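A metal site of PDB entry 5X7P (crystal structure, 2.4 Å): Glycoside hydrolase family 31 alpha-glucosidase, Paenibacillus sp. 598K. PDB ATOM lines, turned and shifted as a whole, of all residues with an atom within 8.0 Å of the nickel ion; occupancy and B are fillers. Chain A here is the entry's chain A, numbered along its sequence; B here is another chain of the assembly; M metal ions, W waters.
Of the 18 residues printed, 3 come within 4 Å of the nickel ion.
Water W3 bridges the side-chain carboxylate of Asp 178 and the backbone carbonyl oxygen of Ala 179.
The nickel ion is bound by water W2 (2.1 Å), water W1 (2.2 Å), the side-chain carboxylate of Asp 178 (2.2 Å), a ring nitrogen (NE2) of His 169 (2.3 Å), water W3 (2.3 Å) and a ring nitrogen (NE2) of His 172 (2.4 Å).
NH2 of Arg 151 lies close to ND1 of His 169, at 3.3 Å.
N of Gly 180 lies within hydrogen-bond range of O of His 172 (3.2 Å).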
ATOM      1  N   ILE A 150      -0.704 -13.962  28.480  1.00  0.00           N
ATOM      2  CA  ILE A 150      -1.161 -12.706  27.909  1.00  0.00           C
ATOM      3  C   ILE A 150      -1.070 -12.632  26.403  1.00  0.00           C
ATOM      4  O   ILE A 150      -2.062 -12.302  25.729  1.00  0.00           O
ATOM      5  CB  ILE A 150      -0.478 -11.475  28.523  1.00  0.00           C
ATOM      6  CG1 ILE A 150      -0.796 -11.387  30.044  1.00  0.00           C
ATOM      7  CG2 ILE A 150      -0.943 -10.185  27.868  1.00  0.00           C
ATOM      8  CD1 ILE A 150       0.043 -10.355  30.781  1.00  0.00           C
ATOM      9  N   ARG A 151       0.144 -12.872  25.913  1.00  0.00           N
ATOM     10  CA  ARG A 151       0.490 -12.518  24.555  1.00  0.00           C
ATOM     11  C   ARG A 151       1.646 -13.319  24.005  1.00  0.00           C
ATOM     12  O   ARG A 151       2.406 -13.938  24.771  1.00  0.00           O
ATOM     13  CB  ARG A 151       0.797 -10.999  24.406  1.00  0.00           C
ATOM     14  CG  ARG A 151       1.984 -10.464  25.218  1.00  0.00           C
ATOM     15  CD  ARG A 151       3.307 -10.518  24.482  1.00  0.00           C
ATOM     16  NE  ARG A 151       3.273  -9.610  23.367  1.00  0.00           N
ATOM     17  CZ  ARG A 151       3.669  -8.325  23.369  1.00  0.00           C
ATOM     18  NH1 ARG A 151       4.165  -7.726  24.479  1.00  0.00           N
ATOM     19  NH2 ARG A 151       3.567  -7.638  22.216  1.00  0.00           N
ATOM     20  N   SER A 152       1.718 -13.291  22.678  1.00  0.00           N
ATOM     21  CA  SER A 152       2.859 -13.714  21.908  1.00  0.00           C
ATOM     22  C   SER A 152       3.289 -12.571  20.944  1.00  0.00           C
ATOM     23  O   SER A 152       3.021 -11.376  21.220  1.00  0.00           O
ATOM     24  CB  SER A 152       2.487 -14.986  21.153  1.00  0.00           C
ATOM     25  OG  SER A 152       3.624 -15.492  20.492  1.00  0.00           O
ATOM     26  N   PHE A 153       3.955 -12.905  19.830  1.00  0.00           N
ATOM     27  CA  PHE A 153       4.379 -11.894  18.853  1.00  0.00           C
ATOM     28  C   PHE A 153       4.086 -12.344  17.418  1.00  0.00           C
ATOM     29  O   PHE A 153       4.064 -13.539  17.091  1.00  0.00           O
ATOM     30  CB  PHE A 153       5.859 -11.559  19.023  1.00  0.00           C
ATOM     31  CG  PHE A 153       6.264 -11.397  20.445  1.00  0.00           C
ATOM     32  CD1 PHE A 153       6.558 -12.515  21.212  1.00  0.00           C
ATOM     33  CD2 PHE A 153       6.245 -10.143  21.055  1.00  0.00           C
ATOM     34  CE1 PHE A 153       6.889 -12.373  22.543  1.00  0.00           C
ATOM     35  CE2 PHE A 153       6.578 -10.012  22.413  1.00  0.00           C
ATOM     36  CZ  PHE A 153       6.926 -11.137  23.140  1.00  0.00           C
ATOM     37  N   ASN A 154       3.828 -11.360  16.573  1.00  0.00           N
ATOM     38  CA  ASN A 154       3.416 -11.648  15.234  1.00  0.00           C
ATOM     39  C   ASN A 154       4.565 -11.505  14.265  1.00  0.00           C
ATOM     40  O   ASN A 154       5.659 -11.218  14.672  1.00  0.00           O
ATOM     41  CB  ASN A 154       2.170 -10.841  14.866  1.00  0.00           C
ATOM     42  CG  ASN A 154       2.412  -9.369  14.639  1.00  0.00           C
ATOM     43  OD1 ASN A 154       3.507  -8.905  14.357  1.00  0.00           O
ATOM     44  ND2 ASN A 154       1.321  -8.623  14.694  1.00  0.00           N
ATOM     45  N   GLU A 157       6.342  -7.894  14.169  1.00  0.00           N
ATOM     46  CA  GLU A 157       6.635  -7.281  15.446  1.00  0.00           C
ATOM     47  C   GLU A 157       8.011  -7.653  15.894  1.00  0.00           C
ATOM     48  O   GLU A 157       8.509  -8.699  15.516  1.00  0.00           O
ATOM     49  CB  GLU A 157       5.661  -7.786  16.508  1.00  0.00           C
ATOM     50  CG  GLU A 157       4.409  -6.954  16.651  1.00  0.00           C
ATOM     51  CD  GLU A 157       3.443  -7.499  17.699  1.00  0.00           C
ATOM     52  OE1 GLU A 157       3.468  -8.723  18.044  1.00  0.00           O
ATOM     53  OE2 GLU A 157       2.630  -6.678  18.180  1.00  0.00           O
ATOM     54  N   HIS A 169       0.201  -4.981  27.221  1.00  0.00           N
ATOM     55  CA  HIS A 169      -0.266  -5.309  25.857  1.00  0.00           C
ATOM     56  C   HIS A 169      -1.686  -5.815  26.006  1.00  0.00           C
ATOM     57  O   HIS A 169      -1.972  -6.470  27.001  1.00  0.00           O
ATOM     58  CB  HIS A 169       0.638  -6.358  25.244  1.00  0.00           C
ATOM     59  CG  HIS A 169       0.466  -6.551  23.764  1.00  0.00           C
ATOM     60  ND1 HIS A 169       1.018  -5.691  22.830  1.00  0.00           N
ATOM     61  CD2 HIS A 169      -0.127  -7.555  23.063  1.00  0.00           C
ATOM     62  CE1 HIS A 169       0.738  -6.139  21.618  1.00  0.00           C
ATOM     63  NE2 HIS A 169       0.053  -7.271  21.735  1.00  0.00           N
ATOM     64  N   PRO A 170      -2.586  -5.495  25.072  1.00  0.00           N
ATOM     65  CA  PRO A 170      -3.944  -6.053  25.159  1.00  0.00           C
ATOM     66  C   PRO A 170      -3.960  -7.562  25.031  1.00  0.00           C
ATOM     67  O   PRO A 170      -3.007  -8.145  24.491  1.00  0.00           O
ATOM     68  CB  PRO A 170      -4.688  -5.430  23.979  1.00  0.00           C
ATOM     69  CG  PRO A 170      -3.844  -4.321  23.475  1.00  0.00           C
ATOM     70  CD  PRO A 170      -2.434  -4.574  23.920  1.00  0.00           C
ATOM     71  N   ALA A 171      -5.038  -8.169  25.539  1.00  0.00           N
ATOM     72  CA  ALA A 171      -5.345  -9.591  25.294  1.00  0.00           C
ATOM     73  C   ALA A 171      -6.150  -9.646  24.011  1.00  0.00           C
ATOM     74  O   ALA A 171      -7.244  -9.131  23.934  1.00  0.00           O
ATOM     75  CB  ALA A 171      -6.151 -10.191  26.451  1.00  0.00           C
ATOM     76  N   HIS A 172      -5.568 -10.219  22.979  1.00  0.00           N
ATOM     77  CA  HIS A 172      -6.288 -10.407  21.707  1.00  0.00           C
ATOM     78  C   HIS A 172      -5.765 -11.600  20.923  1.00  0.00           C
ATOM     79  O   HIS A 172      -4.634 -12.036  21.129  1.00  0.00           O
ATOM     80  CB  HIS A 172      -6.203  -9.142  20.854  1.00  0.00           C
ATOM     81  CG  HIS A 172      -4.814  -8.636  20.591  1.00  0.00           C
ATOM     82  ND1 HIS A 172      -4.503  -7.306  20.648  1.00  0.00           N
ATOM     83  CD2 HIS A 172      -3.661  -9.278  20.252  1.00  0.00           C
ATOM     84  CE1 HIS A 172      -3.227  -7.140  20.361  1.00  0.00           C
ATOM     85  NE2 HIS A 172      -2.693  -8.321  20.117  1.00  0.00           N
ATOM     86  N   ALA A 173      -6.585 -12.109  20.018  1.00  0.00           N
ATOM     87  CA  ALA A 173      -6.133 -13.079  19.033  1.00  0.00           C
ATOM     88  C   ALA A 173      -5.002 -12.494  18.192  1.00  0.00           C
ATOM     89  O   ALA A 173      -3.995 -13.158  17.972  1.00  0.00           O
ATOM     90  CB  ALA A 173      -7.281 -13.485  18.126  1.00  0.00           C
ATOM     91  N   GLY A 174      -5.172 -11.250  17.755  1.00  0.00           N
ATOM     92  CA  GLY A 174      -4.166 -10.518  16.962  1.00  0.00           C
ATOM     93  C   GLY A 174      -4.187 -10.951  15.502  1.00  0.00           C
ATOM     94  O   GLY A 174      -5.241 -11.381  14.966  1.00  0.00           O
ATOM     95  N   GLN A 175      -3.012 -10.834  14.870  1.00  0.00           N
ATOM     96  CA  GLN A 175      -2.804 -11.240  13.469  1.00  0.00           C
ATOM     97  C   GLN A 175      -1.395 -11.806  13.221  1.00  0.00           C
ATOM     98  O   GLN A 175      -0.520 -11.663  14.040  1.00  0.00           O
ATOM     99  CB  GLN A 175      -3.010 -10.039  12.551  1.00  0.00           C
ATOM    100  CG  GLN A 175      -2.038  -8.859  12.796  1.00  0.00           C
ATOM    101  CD  GLN A 175      -1.885  -7.914  11.611  1.00  0.00           C
ATOM    102  OE1 GLN A 175      -2.122  -8.256  10.437  1.00  0.00           O
ATOM    103  NE2 GLN A 175      -1.532  -6.694  11.922  1.00  0.00           N
ATOM    104  N   GLY A 177       0.198 -14.684  13.143  1.00  0.00           N
ATOM    105  CA  GLY A 177       0.801 -15.663  14.072  1.00  0.00           C
ATOM    106  C   GLY A 177       0.797 -15.283  15.545  1.00  0.00           C
ATOM    107  O   GLY A 177       1.396 -15.960  16.382  1.00  0.00           O
ATOM    108  N   ASP A 178       0.125 -14.194  15.865  1.00  0.00           N
ATOM    109  CA  ASP A 178      -0.033 -13.767  17.234  1.00  0.00           C
ATOM    110  C   ASP A 178      -0.950 -14.705  17.941  1.00  0.00           C
ATOM    111  O   ASP A 178      -1.741 -15.455  17.345  1.00  0.00           O
ATOM    112  CB  ASP A 178      -0.641 -12.376  17.284  1.00  0.00           C
ATOM    113  CG  ASP A 178      -0.260 -11.568  18.523  1.00  0.00           C
ATOM    114  OD1 ASP A 178       0.348 -12.109  19.481  1.00  0.00           O
ATOM    115  OD2 ASP A 178      -0.604 -10.364  18.503  1.00  0.00           O
ATOM    116  N   ALA A 179      -0.828 -14.664  19.250  1.00  0.00           N
ATOM    117  CA  ALA A 179      -1.722 -15.330  20.114  1.00  0.00           C
ATOM    118  C   ALA A 179      -1.825 -14.504  21.389  1.00  0.00           C
ATOM    119  O   ALA A 179      -0.897 -13.793  21.785  1.00  0.00           O
ATOM    120  CB  ALA A 179      -1.200 -16.729  20.390  1.00  0.00           C
ATOM    121  N   GLY A 180      -2.953 -14.589  22.041  1.00  0.00           N
ATOM    122  CA  GLY A 180      -3.096 -13.912  23.321  1.00  0.00           C
ATOM    123  C   GLY A 180      -4.401 -14.237  23.975  1.00  0.00           C
ATOM    124  O   GLY A 180      -5.266 -14.942  23.388  1.00  0.00           O
ATOM    125  N   TRP B 424     -10.686  -5.501  11.077  1.00  0.00           N
ATOM    126  CA  TRP B 424     -10.296  -6.515  11.984  1.00  0.00           C
ATOM    127  C   TRP B 424     -11.403  -7.561  12.072  1.00  0.00           C
ATOM    128  O   TRP B 424     -12.585  -7.217  11.999  1.00  0.00           O
ATOM    129  CB  TRP B 424     -10.059  -5.899  13.325  1.00  0.00           C
ATOM    130  CG  TRP B 424      -8.700  -5.354  13.478  1.00  0.00           C
ATOM    131  CD1 TRP B 424      -8.295  -4.072  13.247  1.00  0.00           C
ATOM    132  CD2 TRP B 424      -7.546  -6.064  13.986  1.00  0.00           C
ATOM    133  NE1 TRP B 424      -6.956  -3.930  13.564  1.00  0.00           N
ATOM    134  CE2 TRP B 424      -6.478  -5.139  14.013  1.00  0.00           C
ATOM    135  CE3 TRP B 424      -7.319  -7.372  14.399  1.00  0.00           C
ATOM    136  CZ2 TRP B 424      -5.183  -5.494  14.427  1.00  0.00           C
ATOM    137  CZ3 TRP B 424      -6.046  -7.729  14.815  1.00  0.00           C
ATOM    138  CH2 TRP B 424      -4.989  -6.789  14.834  1.00  0.00           C
HETATM  139 NI    NI M   1      -0.337  -8.859  20.088  1.00  0.00          NI
HETATM  140  O   HOH W   1       1.779  -9.367  20.128  1.00  0.00           O
HETATM  141  O   HOH W   2       0.121  -7.483  18.609  1.00  0.00           O
HETATM  142  O   HOH W   3      -0.736 -10.598  21.590  1.00  0.00           O
